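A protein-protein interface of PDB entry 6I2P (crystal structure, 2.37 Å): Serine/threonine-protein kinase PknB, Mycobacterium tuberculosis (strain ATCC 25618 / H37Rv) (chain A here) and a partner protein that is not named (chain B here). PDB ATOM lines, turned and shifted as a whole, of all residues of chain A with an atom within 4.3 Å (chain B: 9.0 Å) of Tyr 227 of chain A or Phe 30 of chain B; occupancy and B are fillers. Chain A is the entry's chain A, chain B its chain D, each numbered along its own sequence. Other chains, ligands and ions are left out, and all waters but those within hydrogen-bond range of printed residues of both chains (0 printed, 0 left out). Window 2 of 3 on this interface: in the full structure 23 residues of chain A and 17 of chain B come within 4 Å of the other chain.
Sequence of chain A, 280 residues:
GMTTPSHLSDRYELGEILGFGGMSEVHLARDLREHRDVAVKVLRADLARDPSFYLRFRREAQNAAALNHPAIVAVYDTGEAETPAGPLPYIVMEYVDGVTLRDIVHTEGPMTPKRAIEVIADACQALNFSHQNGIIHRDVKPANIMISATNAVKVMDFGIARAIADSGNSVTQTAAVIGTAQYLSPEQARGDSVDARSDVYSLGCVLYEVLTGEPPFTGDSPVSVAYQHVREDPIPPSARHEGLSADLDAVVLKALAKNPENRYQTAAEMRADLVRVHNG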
ATOM      1  N   ALA A 189       5.606  18.044 -19.244  1.00  0.00           N
ATOM      2  CA  ALA A 189       6.182  18.314 -20.559  1.00  0.00           C
ATOM      3  C   ALA A 189       7.387  17.419 -20.836  1.00  0.00           C
ATOM      4  O   ALA A 189       7.588  17.003 -21.975  1.00  0.00           O
ATOM      5  CB  ALA A 189       6.576  19.785 -20.666  1.00  0.00           C
ATOM      6  N   VAL A 223       5.783  23.198 -28.282  1.00  0.00           N
ATOM      7  CA  VAL A 223       7.181  22.876 -27.946  1.00  0.00           C
ATOM      8  C   VAL A 223       7.838  24.109 -27.304  1.00  0.00           C
ATOM      9  O   VAL A 223       8.519  23.975 -26.287  1.00  0.00           O
ATOM     10  CB  VAL A 223       8.011  22.383 -29.175  1.00  0.00           C
ATOM     11  CG1 VAL A 223       9.402  21.910 -28.757  1.00  0.00           C
ATOM     12  CG2 VAL A 223       7.294  21.284 -29.944  1.00  0.00           C
ATOM     13  N   SER A 224       7.627  25.299 -27.907  1.00  0.00           N
ATOM     14  CA  SER A 224       8.165  26.581 -27.446  1.00  0.00           C
ATOM     15  C   SER A 224       7.638  26.945 -26.057  1.00  0.00           C
ATOM     16  O   SER A 224       8.407  27.427 -25.221  1.00  0.00           O
ATOM     17  CB  SER A 224       7.847  27.686 -28.451  1.00  0.00           C
ATOM     18  OG  SER A 224       8.513  28.895 -28.118  1.00  0.00           O
ATOM     19  N   VAL A 225       6.337  26.689 -25.809  1.00  0.00           N
ATOM     20  CA  VAL A 225       5.671  26.945 -24.526  1.00  0.00           C
ATOM     21  C   VAL A 225       6.205  25.966 -23.465  1.00  0.00           C
ATOM     22  O   VAL A 225       6.525  26.392 -22.349  1.00  0.00           O
ATOM     23  CB  VAL A 225       4.119  26.913 -24.640  1.00  0.00           C
ATOM     24  CG1 VAL A 225       3.454  27.326 -23.328  1.00  0.00           C
ATOM     25  CG2 VAL A 225       3.625  27.799 -25.782  1.00  0.00           C
ATOM     26  N   ALA A 226       6.331  24.665 -23.826  1.00  0.00           N
ATOM     27  CA  ALA A 226       6.858  23.615 -22.945  1.00  0.00           C
ATOM     28  C   ALA A 226       8.301  23.917 -22.541  1.00  0.00           C
ATOM     29  O   ALA A 226       8.656  23.709 -21.383  1.00  0.00           O
ATOM     30  CB  ALA A 226       6.776  22.258 -23.621  1.00  0.00           C
ATOM     31  N   TYR A 227       9.112  24.444 -23.493  1.00  0.00           N
ATOM     32  CA  TYR A 227      10.507  24.857 -23.300  1.00  0.00           C
ATOM     33  C   TYR A 227      10.559  25.968 -22.252  1.00  0.00           C
ATOM     34  O   TYR A 227      11.375  25.899 -21.329  1.00  0.00           O
ATOM     35  CB  TYR A 227      11.100  25.335 -24.640  1.00  0.00           C
ATOM     36  CG  TYR A 227      12.569  25.696 -24.601  1.00  0.00           C
ATOM     37  CD1 TYR A 227      13.549  24.741 -24.855  1.00  0.00           C
ATOM     38  CD2 TYR A 227      12.979  27.009 -24.381  1.00  0.00           C
ATOM     39  CE1 TYR A 227      14.904  25.078 -24.862  1.00  0.00           C
ATOM     40  CE2 TYR A 227      14.331  27.353 -24.362  1.00  0.00           C
ATOM     41  CZ  TYR A 227      15.289  26.385 -24.611  1.00  0.00           C
ATOM     42  OH  TYR A 227      16.623  26.723 -24.604  1.00  0.00           O
ATOM     43  N   GLN A 228       9.665  26.971 -22.391  1.00  0.00           N
ATOM     44  CA  GLN A 228       9.529  28.110 -21.485  1.00  0.00           C
ATOM     45  C   GLN A 228       9.162  27.650 -20.069  1.00  0.00           C
ATOM     46  O   GLN A 228       9.769  28.129 -19.111  1.00  0.00           O
ATOM     47  CB  GLN A 228       8.498  29.121 -22.019  1.00  0.00           C
ATOM     48  CG  GLN A 228       9.017  30.002 -23.149  1.00  0.00           C
ATOM     49  CD  GLN A 228       7.965  30.970 -23.624  1.00  0.00           C
ATOM     50  OE1 GLN A 228       7.780  32.051 -23.054  1.00  0.00           O
ATOM     51  NE2 GLN A 228       7.251  30.606 -24.681  1.00  0.00           N
ATOM     52  N   HIS A 229       8.209  26.692 -19.941  1.00  0.00           N
ATOM     53  CA  HIS A 229       7.789  26.129 -18.654  1.00  0.00           C
ATOM     54  C   HIS A 229       8.977  25.492 -17.931  1.00  0.00           C
ATOM     55  O   HIS A 229       9.087  25.611 -16.717  1.00  0.00           O
ATOM     56  CB  HIS A 229       6.694  25.056 -18.842  1.00  0.00           C
ATOM     57  CG  HIS A 229       5.297  25.587 -18.967  1.00  0.00           C
ATOM     58  ND1 HIS A 229       4.685  26.274 -17.931  1.00  0.00           N
ATOM     59  CD2 HIS A 229       4.412  25.450 -19.980  1.00  0.00           C
ATOM     60  CE1 HIS A 229       3.468  26.564 -18.361  1.00  0.00           C
ATOM     61  NE2 HIS A 229       3.258  26.085 -19.587  1.00  0.00           N
ATOM     62  N   VAL A 230       9.864  24.826 -18.687  1.00  0.00           N
ATOM     63  CA  VAL A 230      11.033  24.115 -18.176  1.00  0.00           C
ATOM     64  C   VAL A 230      12.216  25.055 -17.858  1.00  0.00           C
ATOM     65  O   VAL A 230      12.762  24.966 -16.757  1.00  0.00           O
ATOM     66  CB  VAL A 230      11.430  22.949 -19.141  1.00  0.00           C
ATOM     67  CG1 VAL A 230      12.812  22.368 -18.823  1.00  0.00           C
ATOM     68  CG2 VAL A 230      10.371  21.846 -19.150  1.00  0.00           C
ATOM     69  N   ARG A 231      12.593  25.953 -18.786  1.00  0.00           N
ATOM     70  CA  ARG A 231      13.788  26.790 -18.619  1.00  0.00           C
ATOM     71  C   ARG A 231      13.555  28.294 -18.380  1.00  0.00           C
ATOM     72  O   ARG A 231      14.274  28.873 -17.563  1.00  0.00           O
ATOM     73  CB  ARG A 231      14.737  26.608 -19.805  1.00  0.00           C
ATOM     74  CG  ARG A 231      15.102  25.157 -20.059  1.00  0.00           C
ATOM     75  CD  ARG A 231      15.648  24.970 -21.429  1.00  0.00           C
ATOM     76  NE  ARG A 231      15.910  23.561 -21.711  1.00  0.00           N
ATOM     77  CZ  ARG A 231      17.116  23.009 -21.670  1.00  0.00           C
ATOM     78  NH1 ARG A 231      18.179  23.743 -21.366  1.00  0.00           N
ATOM     79  NH2 ARG A 231      17.271  21.720 -21.942  1.00  0.00           N
ATOM     80  N   GLU A 232      12.615  28.938 -19.100  1.00  0.00           N
ATOM     81  CA  GLU A 232      12.390  30.381 -18.958  1.00  0.00           C
ATOM     82  C   GLU A 232      11.646  30.753 -17.682  1.00  0.00           C
ATOM     83  O   GLU A 232      10.603  30.174 -17.385  1.00  0.00           O
ATOM     84  CB  GLU A 232      11.688  30.963 -20.194  1.00  0.00           C
ATOM     85  N   ARG B  27      14.216  19.915 -28.656  1.00  0.00           N
ATOM     86  CA  ARG B  27      12.876  19.355 -28.832  1.00  0.00           C
ATOM     87  C   ARG B  27      12.767  17.912 -28.340  1.00  0.00           C
ATOM     88  O   ARG B  27      11.697  17.515 -27.882  1.00  0.00           O
ATOM     89  CB  ARG B  27      12.423  19.452 -30.297  1.00  0.00           C
ATOM     90  N   ALA B  28      13.871  17.137 -28.427  1.00  0.00           N
ATOM     91  CA  ALA B  28      13.947  15.727 -28.015  1.00  0.00           C
ATOM     92  C   ALA B  28      13.722  15.488 -26.511  1.00  0.00           C
ATOM     93  O   ALA B  28      13.296  14.396 -26.127  1.00  0.00           O
ATOM     94  CB  ALA B  28      15.271  15.125 -28.456  1.00  0.00           C
ATOM     95  N   ASP B  29      13.985  16.515 -25.679  1.00  0.00           N
ATOM     96  CA  ASP B  29      13.842  16.500 -24.217  1.00  0.00           C
ATOM     97  C   ASP B  29      12.375  16.379 -23.742  1.00  0.00           C
ATOM     98  O   ASP B  29      12.124  16.018 -22.593  1.00  0.00           O
ATOM     99  CB  ASP B  29      14.492  17.769 -23.633  1.00  0.00           C
ATOM    100  CG  ASP B  29      14.665  17.762 -22.131  1.00  0.00           C
ATOM    101  OD1 ASP B  29      15.564  17.044 -21.641  1.00  0.00           O
ATOM    102  OD2 ASP B  29      13.911  18.485 -21.447  1.00  0.00           O
ATOM    103  N   PHE B  30      11.418  16.668 -24.626  1.00  0.00           N
ATOM    104  CA  PHE B  30       9.995  16.618 -24.296  1.00  0.00           C
ATOM    105  C   PHE B  30       9.327  15.357 -24.796  1.00  0.00           C
ATOM    106  O   PHE B  30       9.947  14.597 -25.533  1.00  0.00           O
ATOM    107  CB  PHE B  30       9.288  17.874 -24.825  1.00  0.00           C
ATOM    108  CG  PHE B  30       9.940  19.143 -24.338  1.00  0.00           C
ATOM    109  CD1 PHE B  30       9.759  19.578 -23.031  1.00  0.00           C
ATOM    110  CD2 PHE B  30      10.780  19.873 -25.168  1.00  0.00           C
ATOM    111  CE1 PHE B  30      10.390  20.732 -22.571  1.00  0.00           C
ATOM    112  CE2 PHE B  30      11.412  21.028 -24.706  1.00  0.00           C
ATOM    113  CZ  PHE B  30      11.220  21.444 -23.408  1.00  0.00           C
ATOM    114  N   LEU B  31       8.083  15.103 -24.360  1.00  0.00           N
ATOM    115  CA  LEU B  31       7.314  13.948 -24.833  1.00  0.00           C
ATOM    116  C   LEU B  31       6.848  14.229 -26.267  1.00  0.00           C
ATOM    117  O   LEU B  31       6.616  15.387 -26.626  1.00  0.00           O
ATOM    118  CB  LEU B  31       6.116  13.637 -23.911  1.00  0.00           C
ATOM    119  CG  LEU B  31       6.445  13.076 -22.512  1.00  0.00           C
ATOM    120  CD1 LEU B  31       5.238  13.134 -21.620  1.00  0.00           C
ATOM    121  CD2 LEU B  31       6.953  11.634 -22.578  1.00  0.00           C
ATOM    122  N   SER B  32       6.751  13.167 -27.077  1.00  0.00           N
ATOM    123  CA  SER B  32       6.386  13.168 -28.495  1.00  0.00           C
ATOM    124  C   SER B  32       5.128  13.961 -28.862  1.00  0.00           C
ATOM    125  O   SER B  32       5.107  14.581 -29.929  1.00  0.00           O
ATOM    126  CB  SER B  32       6.249  11.740 -29.004  1.00  0.00           C
ATOM    127  OG  SER B  32       7.352  10.926 -28.647  1.00  0.00           O
ATOM    128  N   GLU B  33       4.090  13.938 -27.996  1.00  0.00           N
ATOM    129  CA  GLU B  33       2.805  14.636 -28.187  1.00  0.00           C
ATOM    130  C   GLU B  33       2.972  16.133 -28.421  1.00  0.00           C
ATOM    131  O   GLU B  33       2.161  16.729 -29.127  1.00  0.00           O
ATOM    132  CB  GLU B  33       1.854  14.400 -26.998  1.00  0.00           C
ATOM    133  CG  GLU B  33       1.290  12.990 -26.911  1.00  0.00           C
ATOM    134  CD  GLU B  33       2.185  11.907 -26.333  1.00  0.00           C
ATOM    135  OE1 GLU B  33       3.329  12.209 -25.922  1.00  0.00           O
ATOM    136  OE2 GLU B  33       1.735  10.741 -26.297  1.00  0.00           O
ATOM    137  N   LEU B  34       4.031  16.736 -27.854  1.00  0.00           N
ATOM    138  CA  LEU B  34       4.321  18.157 -28.026  1.00  0.00           C
ATOM    139  C   LEU B  34       4.748  18.525 -29.460  1.00  0.00           C
ATOM    140  O   LEU B  34       4.711  19.706 -29.815  1.00  0.00           O
ATOM    141  CB  LEU B  34       5.337  18.640 -26.988  1.00  0.00           C
ATOM    142  CG  LEU B  34       4.764  18.888 -25.594  1.00  0.00           C
ATOM    143  CD1 LEU B  34       5.810  18.712 -24.530  1.00  0.00           C
ATOM    144  CD2 LEU B  34       4.110  20.246 -25.488  1.00  0.00           C
ATOM    145  N   ASP B  35       5.068  17.499 -30.293  1.00  0.00           N
ATOM    146  CA  ASP B  35       5.485  17.558 -31.703  1.00  0.00           C
ATOM    147  C   ASP B  35       6.876  18.157 -31.876  1.00  0.00           C
ATOM    148  O   ASP B  35       7.841  17.418 -32.061  1.00  0.00           O
ATOM    149  CB  ASP B  35       4.447  18.262 -32.605  1.00  0.00           C
ATOM    150  CG  ASP B  35       3.021  17.775 -32.426  1.00  0.00           C
ATOM    151  OD1 ASP B  35       2.727  16.631 -32.838  1.00  0.00           O
ATOM    152  OD2 ASP B  35       2.196  18.542 -31.884  1.00  0.00           O
ATOM    153  N   ARG B  63      14.058   7.983 -17.999  1.00  0.00           N
ATOM    154  CA  ARG B  63      13.670   8.939 -16.953  1.00  0.00           C
ATOM    155  C   ARG B  63      12.367   8.581 -16.220  1.00  0.00           C
ATOM    156  O   ARG B  63      11.658   7.659 -16.617  1.00  0.00           O
ATOM    157  CB  ARG B  63      13.617  10.383 -17.501  1.00  0.00           C
ATOM    158  CG  ARG B  63      12.637  10.612 -18.650  1.00  0.00           C
ATOM    159  CD  ARG B  63      12.515  12.086 -19.007  1.00  0.00           C
ATOM    160  NE  ARG B  63      13.685  12.560 -19.742  1.00  0.00           N
ATOM    161  CZ  ARG B  63      13.771  13.737 -20.353  1.00  0.00           C
ATOM    162  NH1 ARG B  63      14.877  14.072 -21.001  1.00  0.00           N
ATOM    163  NH2 ARG B  63      12.749  14.583 -20.328  1.00  0.00           N
ATOM    164  N   TYR B 121       5.684   5.617 -30.185  1.00  0.00           N
ATOM    165  CA  TYR B 121       6.578   6.549 -30.863  1.00  0.00           C
ATOM    166  C   TYR B 121       7.998   6.015 -30.885  1.00  0.00           C
ATOM    167  O   TYR B 121       8.472   5.461 -29.892  1.00  0.00           O
ATOM    168  CB  TYR B 121       6.545   7.936 -30.189  1.00  0.00           C
ATOM    169  CG  TYR B 121       5.159   8.535 -30.057  1.00  0.00           C
ATOM    170  CD1 TYR B 121       4.336   8.212 -28.981  1.00  0.00           C
ATOM    171  CD2 TYR B 121       4.694   9.471 -30.974  1.00  0.00           C
ATOM    172  CE1 TYR B 121       3.061   8.760 -28.854  1.00  0.00           C
ATOM    173  CE2 TYR B 121       3.429  10.046 -30.844  1.00  0.00           C
ATOM    174  CZ  TYR B 121       2.613   9.681 -29.784  1.00  0.00           C
ATOM    175  OH  TYR B 121       1.365  10.235 -29.644  1.00  0.00           O
ATOM    176  N   ASN B 123      11.714   7.533 -31.810  1.00  0.00           N
ATOM    177  CA  ASN B 123      12.480   8.768 -32.016  1.00  0.00           C
ATOM    178  C   ASN B 123      11.545   9.988 -32.210  1.00  0.00           C
ATOM    179  O   ASN B 123      11.746  10.801 -33.121  1.00  0.00           O
ATOM    180  CB  ASN B 123      13.523   8.606 -33.144  1.00  0.00           C
ATOM    181  CG  ASN B 123      14.524   7.493 -32.903  1.00  0.00           C
ATOM    182  OD1 ASN B 123      14.840   7.126 -31.764  1.00  0.00           O
ATOM    183  ND2 ASN B 123      15.048   6.925 -33.977  1.00  0.00           N
ATOM    184  N   ARG B 124      10.494  10.077 -31.336  1.00  0.00           N
ATOM    185  CA  ARG B 124       9.463  11.132 -31.284  1.00  0.00           C
ATOM    186  C   ARG B 124       8.397  11.041 -32.381  1.00  0.00           C
ATOM    187  O   ARG B 124       7.456  11.838 -32.381  1.00  0.00           O
ATOM    188  CB  ARG B 124      10.085  12.539 -31.323  1.00  0.00           C
ATOM    189  CG  ARG B 124      10.965  12.911 -30.148  1.00  0.00           C
ATOM    190  CD  ARG B 124      11.439  14.350 -30.306  1.00  0.00           C
ATOM    191  NE  ARG B 124      10.329  15.308 -30.405  1.00  0.00           N
ATOM    192  CZ  ARG B 124       9.634  15.759 -29.366  1.00  0.00           C
ATOM    193  NH1 ARG B 124       8.646  16.623 -29.545  1.00  0.00           N
ATOM    194  NH2 ARG B 124       9.930  15.358 -28.138  1.00  0.00           N
ATOM    195  N   GLU B 137      14.924   5.492 -29.380  1.00  0.00           N
ATOM    196  CA  GLU B 137      14.066   5.800 -28.244  1.00  0.00           C
ATOM    197  C   GLU B 137      12.616   5.424 -28.542  1.00  0.00           C
ATOM    198  O   GLU B 137      12.049   5.857 -29.544  1.00  0.00           O
ATOM    199  CB  GLU B 137      14.202   7.269 -27.819  1.00  0.00           C
ATOM    200  CG  GLU B 137      15.496   7.537 -27.056  1.00  0.00           C
ATOM    201  CD  GLU B 137      15.540   8.785 -26.195  1.00  0.00           C
ATOM    202  OE1 GLU B 137      16.479   9.591 -26.376  1.00  0.00           O
ATOM    203  OE2 GLU B 137      14.653   8.949 -25.326  1.00  0.00           O
ATOM    204  N   GLN B 139       8.721   5.414 -27.110  1.00  0.00           N
ATOM    205  CA  GLN B 139       7.795   6.024 -26.164  1.00  0.00           C
ATOM    206  C   GLN B 139       6.495   5.248 -26.116  1.00  0.00           C
ATOM    207  O   GLN B 139       5.787   5.145 -27.121  1.00  0.00           O
ATOM    208  CB  GLN B 139       7.561   7.519 -26.445  1.00  0.00           C
ATOM    209  CG  GLN B 139       6.983   8.256 -25.240  1.00  0.00           C
ATOM    210  CD  GLN B 139       6.372   9.586 -25.587  1.00  0.00           C
ATOM    211  OE1 GLN B 139       7.053  10.539 -25.974  1.00  0.00           O
ATOM    212  NE2 GLN B 139       5.068   9.684 -25.432  1.00  0.00           N
ATOM    213  N   LYS B 142       4.054   7.399 -20.915  1.00  0.00           N
ATOM    214  CA  LYS B 142       4.988   8.403 -20.411  1.00  0.00           C
ATOM    215  C   LYS B 142       6.383   7.769 -20.261  1.00  0.00           C
ATOM    216  O   LYS B 142       7.295   8.423 -19.757  1.00  0.00           O
ATOM    217  CB  LYS B 142       4.507   9.000 -19.071  1.00  0.00           C
ATOM    218  CG  LYS B 142       3.265   9.875 -19.162  1.00  0.00           C
ATOM    219  CD  LYS B 142       2.926  10.454 -17.793  1.00  0.00           C
ATOM    220  CE  LYS B 142       1.592   9.982 -17.263  1.00  0.00           C
ATOM    221  NZ  LYS B 142       1.377  10.413 -15.860  1.00  0.00           N
ATOM    222  N   ARG B 144       9.946   6.516 -21.564  1.00  0.00           N
ATOM    223  CA  ARG B 144      10.940   6.824 -22.584  1.00  0.00           C
ATOM    224  C   ARG B 144      12.010   5.755 -22.454  1.00  0.00           C
ATOM    225  O   ARG B 144      12.846   5.791 -21.549  1.00  0.00           O
ATOM    226  CB  ARG B 144      11.490   8.251 -22.416  1.00  0.00           C
ATOM    227  CG  ARG B 144      10.519   9.327 -22.923  1.00  0.00           C
ATOM    228  CD  ARG B 144      10.958  10.732 -22.555  1.00  0.00           C
ATOM    229  NE  ARG B 144      12.271  11.066 -23.114  1.00  0.00           N
ATOM    230  CZ  ARG B 144      12.561  12.207 -23.730  1.00  0.00           C
ATOM    231  NH1 ARG B 144      11.634  13.142 -23.881  1.00  0.00           N
ATOM    232  NH2 ARG B 144      13.783  12.422 -24.196  1.00  0.00           N
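The backbone carbonyl oxygen (O) of Phe 30 of chain B lies within hydrogen-bond range of the guanidinium group (NH2) of Arg 124 of chain B, at 2.7 Å. The backbone carbonyl oxygen (O) of Phe 30 of chain B is in hydrogen-bond range of the guanidinium group (NH1) of Arg 144 of chain B. O of Asp 35 of chain B sits at hydrogen-bond distance from NH1 of Arg 124 of chain B, 2.8 Å away.
The backbone carbonyl oxygen (O) of Ala 189 of chain A is in hydrogen-bond range of the backbone NH (N) of Leu 31 of chain B (3.1 Å).
Of the 11 printed residues of chain A, 5 touch a printed residue of chain B. Hydrophobic or aromatic side chains of chain A that line the printed part of chain B: Ala 189, Val 223, Ala 226 and Val 230. Hydrophobic or aromatic side chains of chain B that line the printed part of chain A: Phe 30 and Leu 34. Among the printed residues, no Asp or Glu carboxylate lies within 4 Å of a Lys or Arg side-chain nitrogen of the other chain.
Printed residues of chain B within 4 Å of Val 223 of chain A: Leu 34 (3.0 Å) and Asp 35 (3.7 Å). Of chain B, only Phe 30 (3.6 Å) and Leu 34 (3.8 Å) come within 4 Å of Ala 226 of chain A. Glu 232 of chain A touches none of the printed residues of chain B. Phe 30 of chain B touches just these residues of chain A: Ala 189, Ala 226, Tyr 227 and Val 230. Of the printed residues of chain A, Leu 31 of chain B touches Ala 189. Of the printed residues of chain A, Asp 35 of chain B touches Val 223 (3.7 Å). Tyr 121 of chain B touches none of the printed residues of chain A. The nearest residue of chain B that does not touch Tyr 227 of chain A is Arg 27 of chain B (6.2 Å).
Ala 189 of chain A touches Phe 30 of chain B. Leu 34 of chain B touches Ala 189 of chain A (CD1 to O, 3.6 Å). O of Leu 34 of chain B touches CG2 of Val 223 of chain A, at 3.0 Å. CG2 of Val 223 of chain A touches C of Asp 35 of chain B (3.7 Å). Phe 30 of chain B touches Ala 226 of chain A. Leu 34 of chain B touches Ala 226 of chain A (CD1 to CB, 3.8 Å). Phe 30 of chain B touches Tyr 227 of chain A. CG2 of Val 230 of chain A touches CE1 of Phe 30 of chain B, 3.6 Å away.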
